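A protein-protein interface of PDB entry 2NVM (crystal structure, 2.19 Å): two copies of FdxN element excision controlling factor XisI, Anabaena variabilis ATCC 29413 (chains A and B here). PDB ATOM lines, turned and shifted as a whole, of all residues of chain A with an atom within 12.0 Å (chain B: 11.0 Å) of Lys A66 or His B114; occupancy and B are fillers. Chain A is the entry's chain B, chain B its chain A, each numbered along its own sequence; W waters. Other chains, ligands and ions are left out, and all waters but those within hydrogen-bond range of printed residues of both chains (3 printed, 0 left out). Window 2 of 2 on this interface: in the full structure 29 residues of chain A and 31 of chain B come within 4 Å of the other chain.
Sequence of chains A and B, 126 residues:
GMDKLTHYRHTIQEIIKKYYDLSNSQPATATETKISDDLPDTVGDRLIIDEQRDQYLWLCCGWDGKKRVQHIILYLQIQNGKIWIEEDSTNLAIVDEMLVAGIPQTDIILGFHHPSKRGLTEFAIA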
ATOM      1  N   PRO A  40      -6.741  33.477 -19.590  1.00  0.00           N
ATOM      2  CA  PRO A  40      -7.502  32.743 -20.634  1.00  0.00           C
ATOM      3  C   PRO A  40      -6.941  31.443 -21.259  1.00  0.00           C
ATOM      4  O   PRO A  40      -7.737  30.675 -21.783  1.00  0.00           O
ATOM      5  CB  PRO A  40      -7.660  33.807 -21.727  1.00  0.00           C
ATOM      6  CG  PRO A  40      -6.434  34.589 -21.631  1.00  0.00           C
ATOM      7  CD  PRO A  40      -6.146  34.706 -20.168  1.00  0.00           C
ATOM      8  N   ASP A  41      -5.619  31.234 -21.236  1.00  0.00           N
ATOM      9  CA  ASP A  41      -4.960  30.026 -21.814  1.00  0.00           C
ATOM     10  C   ASP A  41      -5.007  28.774 -20.930  1.00  0.00           C
ATOM     11  O   ASP A  41      -4.840  27.668 -21.446  1.00  0.00           O
ATOM     12  CB  ASP A  41      -3.471  30.286 -22.104  1.00  0.00           C
ATOM     13  CG  ASP A  41      -3.212  31.419 -23.066  1.00  0.00           C
ATOM     14  OD1 ASP A  41      -3.937  31.492 -24.051  1.00  0.00           O
ATOM     15  OD2 ASP A  41      -2.236  32.196 -22.849  1.00  0.00           O
ATOM     16  N   THR A  42      -5.187  28.937 -19.611  1.00  0.00           N
ATOM     17  CA  THR A  42      -5.239  27.794 -18.674  1.00  0.00           C
ATOM     18  C   THR A  42      -6.525  26.991 -18.883  1.00  0.00           C
ATOM     19  O   THR A  42      -7.508  27.509 -19.463  1.00  0.00           O
ATOM     20  CB  THR A  42      -5.101  28.222 -17.167  1.00  0.00           C
ATOM     21  OG1 THR A  42      -6.201  29.054 -16.774  1.00  0.00           O
ATOM     22  CG2 THR A  42      -3.801  28.968 -16.925  1.00  0.00           C
ATOM     23  N   VAL A  43      -6.499  25.723 -18.453  1.00  0.00           N
ATOM     24  CA  VAL A  43      -7.673  24.842 -18.556  1.00  0.00           C
ATOM     25  C   VAL A  43      -8.719  25.435 -17.603  1.00  0.00           C
ATOM     26  O   VAL A  43      -8.479  25.533 -16.387  1.00  0.00           O
ATOM     27  CB  VAL A  43      -7.395  23.352 -18.250  1.00  0.00           C
ATOM     28  CG1 VAL A  43      -8.699  22.539 -18.334  1.00  0.00           C
ATOM     29  CG2 VAL A  43      -6.394  22.805 -19.250  1.00  0.00           C
ATOM     30  N   CYS A  61     -11.709  23.833 -21.352  1.00  0.00           N
ATOM     31  CA  CYS A  61     -10.821  24.056 -22.473  1.00  0.00           C
ATOM     32  C   CYS A  61      -9.606  24.890 -22.076  1.00  0.00           C
ATOM     33  O   CYS A  61      -9.727  25.845 -21.298  1.00  0.00           O
ATOM     34  CB  CYS A  61     -11.615  24.723 -23.604  1.00  0.00           C
ATOM     35  SG  CYS A  61     -10.734  25.058 -25.118  1.00  0.00           S
ATOM     36  N   GLY A  62      -8.454  24.494 -22.609  1.00  0.00           N
ATOM     37  CA  GLY A  62      -7.173  25.162 -22.388  1.00  0.00           C
ATOM     38  C   GLY A  62      -5.986  24.253 -22.651  1.00  0.00           C
ATOM     39  O   GLY A  62      -6.105  23.267 -23.400  1.00  0.00           O
ATOM     40  N   TRP A  63      -4.856  24.596 -22.035  1.00  0.00           N
ATOM     41  CA  TRP A  63      -3.597  23.861 -22.181  1.00  0.00           C
ATOM     42  C   TRP A  63      -3.045  23.399 -20.842  1.00  0.00           C
ATOM     43  O   TRP A  63      -2.998  24.192 -19.910  1.00  0.00           O
ATOM     44  CB  TRP A  63      -2.559  24.762 -22.817  1.00  0.00           C
ATOM     45  CG  TRP A  63      -2.945  25.190 -24.140  1.00  0.00           C
ATOM     46  CD1 TRP A  63      -3.631  26.311 -24.460  1.00  0.00           C
ATOM     47  CD2 TRP A  63      -2.710  24.487 -25.354  1.00  0.00           C
ATOM     48  NE1 TRP A  63      -3.831  26.371 -25.810  1.00  0.00           N
ATOM     49  CE2 TRP A  63      -3.282  25.259 -26.394  1.00  0.00           C
ATOM     50  CE3 TRP A  63      -2.065  23.278 -25.675  1.00  0.00           C
ATOM     51  CZ2 TRP A  63      -3.208  24.872 -27.755  1.00  0.00           C
ATOM     52  CZ3 TRP A  63      -1.980  22.891 -27.028  1.00  0.00           C
ATOM     53  CH2 TRP A  63      -2.570  23.678 -28.046  1.00  0.00           C
ATOM     54  N   ASP A  64      -2.656  22.122 -20.774  1.00  0.00           N
ATOM     55  CA  ASP A  64      -2.001  21.503 -19.607  1.00  0.00           C
ATOM     56  C   ASP A  64      -0.541  21.315 -20.107  1.00  0.00           C
ATOM     57  O   ASP A  64      -0.145  20.224 -20.534  1.00  0.00           O
ATOM     58  CB  ASP A  64      -2.729  20.191 -19.245  1.00  0.00           C
ATOM     59  CG  ASP A  64      -2.100  19.443 -18.063  1.00  0.00           C
ATOM     60  OD1 ASP A  64      -1.220  19.975 -17.355  1.00  0.00           O
ATOM     61  OD2 ASP A  64      -2.516  18.288 -17.838  1.00  0.00           O
ATOM     62  N   GLY A  65       0.232  22.410 -20.075  1.00  0.00           N
ATOM     63  CA  GLY A  65       1.613  22.444 -20.595  1.00  0.00           C
ATOM     64  C   GLY A  65       1.505  22.444 -22.118  1.00  0.00           C
ATOM     65  O   GLY A  65       0.945  23.389 -22.688  1.00  0.00           O
ATOM     66  N   LYS A  66       2.026  21.394 -22.765  1.00  0.00           N
ATOM     67  CA  LYS A  66       1.901  21.196 -24.236  1.00  0.00           C
ATOM     68  C   LYS A  66       0.614  20.427 -24.647  1.00  0.00           C
ATOM     69  O   LYS A  66       0.314  20.345 -25.841  1.00  0.00           O
ATOM     70  CB  LYS A  66       3.118  20.448 -24.820  1.00  0.00           C
ATOM     71  CG  LYS A  66       4.441  21.194 -24.821  1.00  0.00           C
ATOM     72  CD  LYS A  66       5.471  20.411 -25.664  1.00  0.00           C
ATOM     73  CE  LYS A  66       6.902  20.991 -25.617  1.00  0.00           C
ATOM     74  NZ  LYS A  66       7.035  22.391 -26.130  1.00  0.00           N
ATOM     75  N   LYS A  67      -0.133  19.890 -23.677  1.00  0.00           N
ATOM     76  CA  LYS A  67      -1.338  19.077 -23.917  1.00  0.00           C
ATOM     77  C   LYS A  67      -2.596  19.950 -24.091  1.00  0.00           C
ATOM     78  O   LYS A  67      -2.970  20.697 -23.180  1.00  0.00           O
ATOM     79  CB  LYS A  67      -1.533  18.105 -22.724  1.00  0.00           C
ATOM     80  CG  LYS A  67      -2.637  17.019 -22.855  1.00  0.00           C
ATOM     81  CD  LYS A  67      -2.963  16.334 -21.478  1.00  0.00           C
ATOM     82  CE  LYS A  67      -1.737  15.723 -20.771  1.00  0.00           C
ATOM     83  N   ARG A  68      -3.248  19.828 -25.249  1.00  0.00           N
ATOM     84  CA  ARG A  68      -4.492  20.539 -25.545  1.00  0.00           C
ATOM     85  C   ARG A  68      -5.651  19.820 -24.869  1.00  0.00           C
ATOM     86  O   ARG A  68      -5.855  18.633 -25.131  1.00  0.00           O
ATOM     87  CB  ARG A  68      -4.771  20.568 -27.065  1.00  0.00           C
ATOM     88  CG  ARG A  68      -6.066  21.288 -27.537  1.00  0.00           C
ATOM     89  CD  ARG A  68      -6.162  22.640 -26.898  1.00  0.00           C
ATOM     90  NE  ARG A  68      -7.150  23.528 -27.471  1.00  0.00           N
ATOM     91  CZ  ARG A  68      -7.493  24.712 -26.960  1.00  0.00           C
ATOM     92  NH1 ARG A  68      -6.918  25.217 -25.864  1.00  0.00           N
ATOM     93  NH2 ARG A  68      -8.406  25.428 -27.590  1.00  0.00           N
ATOM     94  N   VAL A  69      -6.389  20.531 -24.007  1.00  0.00           N
ATOM     95  CA  VAL A  69      -7.560  19.995 -23.290  1.00  0.00           C
ATOM     96  C   VAL A  69      -8.810  20.639 -23.904  1.00  0.00           C
ATOM     97  O   VAL A  69      -8.859  21.855 -24.061  1.00  0.00           O
ATOM     98  CB  VAL A  69      -7.519  20.331 -21.775  1.00  0.00           C
ATOM     99  CG1 VAL A  69      -8.726  19.702 -21.039  1.00  0.00           C
ATOM    100  CG2 VAL A  69      -6.182  19.874 -21.129  1.00  0.00           C
ATOM    101  N   GLN A  70      -9.777  19.818 -24.304  1.00  0.00           N
ATOM    102  CA  GLN A  70     -11.052  20.296 -24.871  1.00  0.00           C
ATOM    103  C   GLN A  70     -12.018  19.146 -24.613  1.00  0.00           C
ATOM    104  O   GLN A  70     -12.153  18.243 -25.427  1.00  0.00           O
ATOM    105  CB  GLN A  70     -10.901  20.652 -26.348  1.00  0.00           C
ATOM    106  CG  GLN A  70     -12.061  21.451 -26.881  1.00  0.00           C
ATOM    107  CD  GLN A  70     -11.835  21.879 -28.332  1.00  0.00           C
ATOM    108  OE1 GLN A  70     -11.381  22.996 -28.588  1.00  0.00           O
ATOM    109  NE2 GLN A  70     -12.066  20.959 -29.271  1.00  0.00           N
ATOM    110  N   TRP B  84     -11.380  34.193 -29.649  1.00  0.00           N
ATOM    111  CA  TRP B  84     -10.534  33.017 -29.454  1.00  0.00           C
ATOM    112  C   TRP B  84     -11.084  31.906 -30.312  1.00  0.00           C
ATOM    113  O   TRP B  84     -12.235  31.513 -30.126  1.00  0.00           O
ATOM    114  CB  TRP B  84     -10.514  32.605 -27.997  1.00  0.00           C
ATOM    115  CG  TRP B  84      -9.757  33.560 -27.186  1.00  0.00           C
ATOM    116  CD1 TRP B  84     -10.096  34.842 -26.907  1.00  0.00           C
ATOM    117  CD2 TRP B  84      -8.530  33.315 -26.526  1.00  0.00           C
ATOM    118  NE1 TRP B  84      -9.143  35.435 -26.120  1.00  0.00           N
ATOM    119  CE2 TRP B  84      -8.163  34.520 -25.865  1.00  0.00           C
ATOM    120  CE3 TRP B  84      -7.693  32.194 -26.416  1.00  0.00           C
ATOM    121  CZ2 TRP B  84      -6.984  34.641 -25.108  1.00  0.00           C
ATOM    122  CZ3 TRP B  84      -6.528  32.307 -25.669  1.00  0.00           C
ATOM    123  CH2 TRP B  84      -6.176  33.533 -25.018  1.00  0.00           C
ATOM    124  N   ILE B  85     -10.288  31.441 -31.275  1.00  0.00           N
ATOM    125  CA  ILE B  85     -10.663  30.304 -32.117  1.00  0.00           C
ATOM    126  C   ILE B  85     -10.099  29.099 -31.349  1.00  0.00           C
ATOM    127  O   ILE B  85      -8.884  28.894 -31.305  1.00  0.00           O
ATOM    128  CB  ILE B  85     -10.144  30.384 -33.536  1.00  0.00           C
ATOM    129  CG1 ILE B  85     -10.551  31.737 -34.155  1.00  0.00           C
ATOM    130  CG2 ILE B  85     -10.679  29.158 -34.353  1.00  0.00           C
ATOM    131  CD1 ILE B  85     -10.136  31.891 -35.510  1.00  0.00           C
ATOM    132  N   GLU B  86     -10.995  28.352 -30.704  1.00  0.00           N
ATOM    133  CA  GLU B  86     -10.615  27.192 -29.876  1.00  0.00           C
ATOM    134  C   GLU B  86     -10.530  25.921 -30.708  1.00  0.00           C
ATOM    135  O   GLU B  86      -9.698  25.071 -30.422  1.00  0.00           O
ATOM    136  CB  GLU B  86     -11.580  27.020 -28.700  1.00  0.00           C
ATOM    137  CG  GLU B  86     -11.827  28.283 -27.833  1.00  0.00           C
ATOM    138  CD  GLU B  86     -10.648  28.773 -26.996  1.00  0.00           C
ATOM    139  OE1 GLU B  86      -9.490  28.359 -27.167  1.00  0.00           O
ATOM    140  OE2 GLU B  86     -10.891  29.629 -26.135  1.00  0.00           O
ATOM    141  N   ILE B 109      -7.338  35.417 -31.764  1.00  0.00           N
ATOM    142  CA  ILE B 109      -6.357  34.518 -31.133  1.00  0.00           C
ATOM    143  C   ILE B 109      -6.654  33.090 -31.585  1.00  0.00           C
ATOM    144  O   ILE B 109      -7.817  32.656 -31.557  1.00  0.00           O
ATOM    145  CB  ILE B 109      -6.428  34.565 -29.575  1.00  0.00           C
ATOM    146  CG1 ILE B 109      -6.264  35.998 -29.033  1.00  0.00           C
ATOM    147  CG2 ILE B 109      -5.353  33.639 -28.924  1.00  0.00           C
ATOM    148  CD1 ILE B 109      -4.947  36.662 -29.379  1.00  0.00           C
ATOM    149  N   LEU B 110      -5.606  32.361 -31.973  1.00  0.00           N
ATOM    150  CA  LEU B 110      -5.705  30.956 -32.374  1.00  0.00           C
ATOM    151  C   LEU B 110      -5.466  30.116 -31.112  1.00  0.00           C
ATOM    152  O   LEU B 110      -4.325  29.750 -30.800  1.00  0.00           O
ATOM    153  CB  LEU B 110      -4.708  30.625 -33.499  1.00  0.00           C
ATOM    154  CG  LEU B 110      -4.874  31.360 -34.837  1.00  0.00           C
ATOM    155  CD1 LEU B 110      -3.870  30.799 -35.854  1.00  0.00           C
ATOM    156  CD2 LEU B 110      -6.292  31.269 -35.391  1.00  0.00           C
ATOM    157  N   GLY B 111      -6.551  29.883 -30.360  1.00  0.00           N
ATOM    158  CA  GLY B 111      -6.543  29.088 -29.106  1.00  0.00           C
ATOM    159  C   GLY B 111      -5.987  27.683 -29.263  1.00  0.00           C
ATOM    160  O   GLY B 111      -5.320  27.167 -28.358  1.00  0.00           O
ATOM    161  N   PHE B 112      -6.243  27.094 -30.432  1.00  0.00           N
ATOM    162  CA  PHE B 112      -5.753  25.757 -30.807  1.00  0.00           C
ATOM    163  C   PHE B 112      -4.247  25.626 -31.033  1.00  0.00           C
ATOM    164  O   PHE B 112      -3.787  24.492 -31.009  1.00  0.00           O
ATOM    165  CB  PHE B 112      -6.529  25.143 -31.996  1.00  0.00           C
ATOM    166  CG  PHE B 112      -6.431  25.946 -33.277  1.00  0.00           C
ATOM    167  CD1 PHE B 112      -5.378  25.745 -34.170  1.00  0.00           C
ATOM    168  CD2 PHE B 112      -7.392  26.933 -33.567  1.00  0.00           C
ATOM    169  CE1 PHE B 112      -5.296  26.511 -35.367  1.00  0.00           C
ATOM    170  CE2 PHE B 112      -7.315  27.713 -34.740  1.00  0.00           C
ATOM    171  CZ  PHE B 112      -6.276  27.502 -35.641  1.00  0.00           C
ATOM    172  N   HIS B 113      -3.504  26.711 -31.308  1.00  0.00           N
ATOM    173  CA  HIS B 113      -2.028  26.695 -31.474  1.00  0.00           C
ATOM    174  C   HIS B 113      -1.424  27.199 -30.182  1.00  0.00           C
ATOM    175  O   HIS B 113      -1.795  28.269 -29.733  1.00  0.00           O
ATOM    176  CB  HIS B 113      -1.538  27.493 -32.709  1.00  0.00           C
ATOM    177  CG  HIS B 113      -1.219  26.617 -33.883  1.00  0.00           C
ATOM    178  ND1 HIS B 113      -2.183  26.099 -34.722  1.00  0.00           N
ATOM    179  CD2 HIS B 113      -0.038  26.109 -34.308  1.00  0.00           C
ATOM    180  CE1 HIS B 113      -1.607  25.331 -35.627  1.00  0.00           C
ATOM    181  NE2 HIS B 113      -0.306  25.316 -35.395  1.00  0.00           N
ATOM    182  N   HIS B 114      -0.548  26.410 -29.543  1.00  0.00           N
ATOM    183  CA  HIS B 114       0.101  26.710 -28.252  1.00  0.00           C
ATOM    184  C   HIS B 114       0.545  28.175 -28.019  1.00  0.00           C
ATOM    185  O   HIS B 114       1.077  28.796 -28.954  1.00  0.00           O
ATOM    186  CB  HIS B 114       1.296  25.759 -28.027  1.00  0.00           C
ATOM    187  CG  HIS B 114       1.685  25.604 -26.599  1.00  0.00           C
ATOM    188  ND1 HIS B 114       2.656  26.374 -26.001  1.00  0.00           N
ATOM    189  CD2 HIS B 114       1.239  24.756 -25.648  1.00  0.00           C
ATOM    190  CE1 HIS B 114       2.781  26.017 -24.740  1.00  0.00           C
ATOM    191  NE2 HIS B 114       1.937  25.031 -24.501  1.00  0.00           N
ATOM    192  N   PRO B 115       0.258  28.757 -26.813  1.00  0.00           N
ATOM    193  CA  PRO B 115       0.690  30.134 -26.448  1.00  0.00           C
ATOM    194  C   PRO B 115       2.126  30.544 -26.819  1.00  0.00           C
ATOM    195  O   PRO B 115       2.358  31.719 -27.165  1.00  0.00           O
ATOM    196  CB  PRO B 115       0.528  30.145 -24.927  1.00  0.00           C
ATOM    197  CG  PRO B 115      -0.627  29.325 -24.700  1.00  0.00           C
ATOM    198  CD  PRO B 115      -0.585  28.207 -25.733  1.00  0.00           C
ATOM    199  N   SER B 116       3.054  29.585 -26.710  1.00  0.00           N
ATOM    200  CA  SER B 116       4.481  29.755 -27.078  1.00  0.00           C
ATOM    201  C   SER B 116       4.743  30.246 -28.521  1.00  0.00           C
ATOM    202  O   SER B 116       5.750  30.931 -28.742  1.00  0.00           O
ATOM    203  CB  SER B 116       5.254  28.445 -26.861  1.00  0.00           C
ATOM    204  OG  SER B 116       4.728  27.400 -27.651  1.00  0.00           O
ATOM    205  N   LYS B 117       3.867  29.876 -29.475  1.00  0.00           N
ATOM    206  CA  LYS B 117       3.979  30.295 -30.899  1.00  0.00           C
ATOM    207  C   LYS B 117       3.317  31.658 -31.293  1.00  0.00           C
ATOM    208  O   LYS B 117       3.379  32.065 -32.473  1.00  0.00           O
ATOM    209  CB  LYS B 117       3.443  29.212 -31.846  1.00  0.00           C
ATOM    210  CG  LYS B 117       4.149  27.864 -31.860  1.00  0.00           C
ATOM    211  CD  LYS B 117       3.504  26.809 -30.991  1.00  0.00           C
ATOM    212  CE  LYS B 117       4.142  25.438 -31.259  1.00  0.00           C
ATOM    213  NZ  LYS B 117       3.474  24.315 -30.532  1.00  0.00           N
ATOM    214  N   ARG B 118       2.758  32.387 -30.326  1.00  0.00           N
ATOM    215  CA  ARG B 118       2.052  33.662 -30.588  1.00  0.00           C
ATOM    216  C   ARG B 118       2.848  34.929 -30.257  1.00  0.00           C
ATOM    217  O   ARG B 118       2.677  35.935 -30.943  1.00  0.00           O
ATOM    218  CB  ARG B 118       0.764  33.690 -29.773  1.00  0.00           C
ATOM    219  CG  ARG B 118      -0.157  32.480 -29.963  1.00  0.00           C
ATOM    220  CD  ARG B 118      -1.288  32.578 -28.976  1.00  0.00           C
ATOM    221  NE  ARG B 118      -1.976  31.310 -28.782  1.00  0.00           N
ATOM    222  CZ  ARG B 118      -2.837  31.058 -27.788  1.00  0.00           C
ATOM    223  NH1 ARG B 118      -3.178  31.993 -26.890  1.00  0.00           N
ATOM    224  NH2 ARG B 118      -3.375  29.848 -27.682  1.00  0.00           N
ATOM    225  N   GLY B 119       3.663  34.889 -29.195  1.00  0.00           N
ATOM    226  CA  GLY B 119       4.462  36.038 -28.755  1.00  0.00           C
ATOM    227  C   GLY B 119       5.646  36.354 -29.643  1.00  0.00           C
ATOM    228  O   GLY B 119       6.500  37.184 -29.291  1.00  0.00           O
HETATM  229  O   HOH W   1      -5.200  29.359 -25.208  1.00  0.00           O
HETATM  230  O   HOH W   2      -7.681  28.296 -25.055  1.00  0.00           O
HETATM  231  O   HOH W   3      -8.617  22.608 -29.990  1.00  0.00           O
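NE1 of Trp A63 sits at hydrogen-bond distance from O of Gly B111, 3.1 Å away. The backbone carbonyl oxygen of Gly A65 sits at hydrogen-bond distance from a ring nitrogen (NE2) of His B114, at 2.6 Å. The backbone carbonyl oxygen of Glu B86 lies close to the side-chain amide oxygen of Gln A70, at 3.2 Å. NH2 of Arg A68 is in salt-bridge range of OE1 of Glu B86, at 3.2 Å. The guanidinium group (NH1) of Arg B118 lies within salt-bridge range of the side-chain carboxylate (OD1) of Asp A41, at 3.0 Å.
The backbone carbonyl oxygen of Leu B110 sits at hydrogen-bond distance from the guanidinium group of Arg B118 (3.3 Å). N of Phe B112 is in hydrogen-bond range of O of Ile B85 (3.3 Å). The backbone carbonyl oxygen of Gly B111 sits at hydrogen-bond distance from the guanidinium group of Arg B118, at 3.4 Å. The side-chain sulfur (SG) of Cys A61 sits at hydrogen-bond distance from the guanidinium group (NH2) of Arg A68, at 3.4 Å. The side-chain hydroxyl of Ser B116 sits at hydrogen-bond distance from a ring nitrogen (ND1) of His B114 (2.8 Å). The backbone NH of Trp A63 lies within hydrogen-bond range of the backbone carbonyl oxygen of Asp A41, at 3.1 Å.
Pro A40 touches Trp B84 (CG to CZ2, 3.5 Å). CG of Asp A41 touches CG of Pro B115, 3.7 Å away. Phe B112 touches Trp A63 (O to CH2, 3.3 Å). Trp A63 touches His B113. Trp A63 touches His B114. Pro B115 touches Trp A63. NE1 of Trp A63 touches NH2 of Arg B118, at 3.98 Å. NE2 of His B114 touches CA of Lys A66, 3.8 Å away. Arg A68 touches Gly B111 (NH1 to O, 3.5 Å). Arg A68 touches Phe B112.
Cys A61 touches none of the printed residues of chain B. Asp A64 touches none of the printed residues of chain B. Of the printed residues of chain B, Gly A65 touches His B114. Lys A66 touches just one residue of chain B: His B114. Of the printed residues of chain B, Arg A68 touches Glu B86 (3.1 Å), Gly B111 (3.5 Å) and Phe B112 (3.9 Å). Of chain A, only Trp A63 (3.1 Å) and Arg A68 (3.5 Å) come within 4 Å of Gly B111. Of the printed residues of chain A, Phe B112 touches Trp A63 and Arg A68. Of the printed residues of chain A, His B113 touches Trp A63 (3.8 Å). Of chain A, only Asp A41 (3.7 Å) and Trp A63 (3.7 Å) come within 4 Å of Pro B115. No residue of chain A comes within 4 Å of Ser B116. No residue of chain A comes within 4 Å of Lys B117. Arg B118 touches just these residues of chain A: Asp A41 and Trp A63. The nearest residue of chain B that does not touch Lys A66 is Ser B116 (5.7 Å). The nearest printed residue of chain B that does not touch Gln A70 is Phe B112 (6.3 Å).
Printed residues of chain B that touch a printed residue of chain A: Trp B84, Glu B86, Gly B111, Phe B112, His B113, His B114, Pro B115 and Arg B118. Hydrophobic or aromatic side chains of chain B within 4 Å of the printed part of chain A: Trp B84, His B114 and Pro B115. Along chain B the printed residues that touch a printed residue of chain A span positions 84 to 118.
No position is printed for both chains. Of the 16 pairs that touch across the chains among the printed residues, none has its exchanged pair printed and touching as well.
Water W3 lies within hydrogen-bond range of O of Glu B86 (2.7 Å), NE of Arg A68 (3.1 Å) and OE1 of Gln A70 (3.1 Å). Water W1 lies within hydrogen-bond range of OD1 of Asp A41 (2.7 Å), NH2 of Arg B118 (3.1 Å) and NE1 of Trp A63 (3.3 Å). Water W2 bridges OE1 of Glu B86 (2.8 Å) and NH1 of Arg A68 (3.3 Å).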
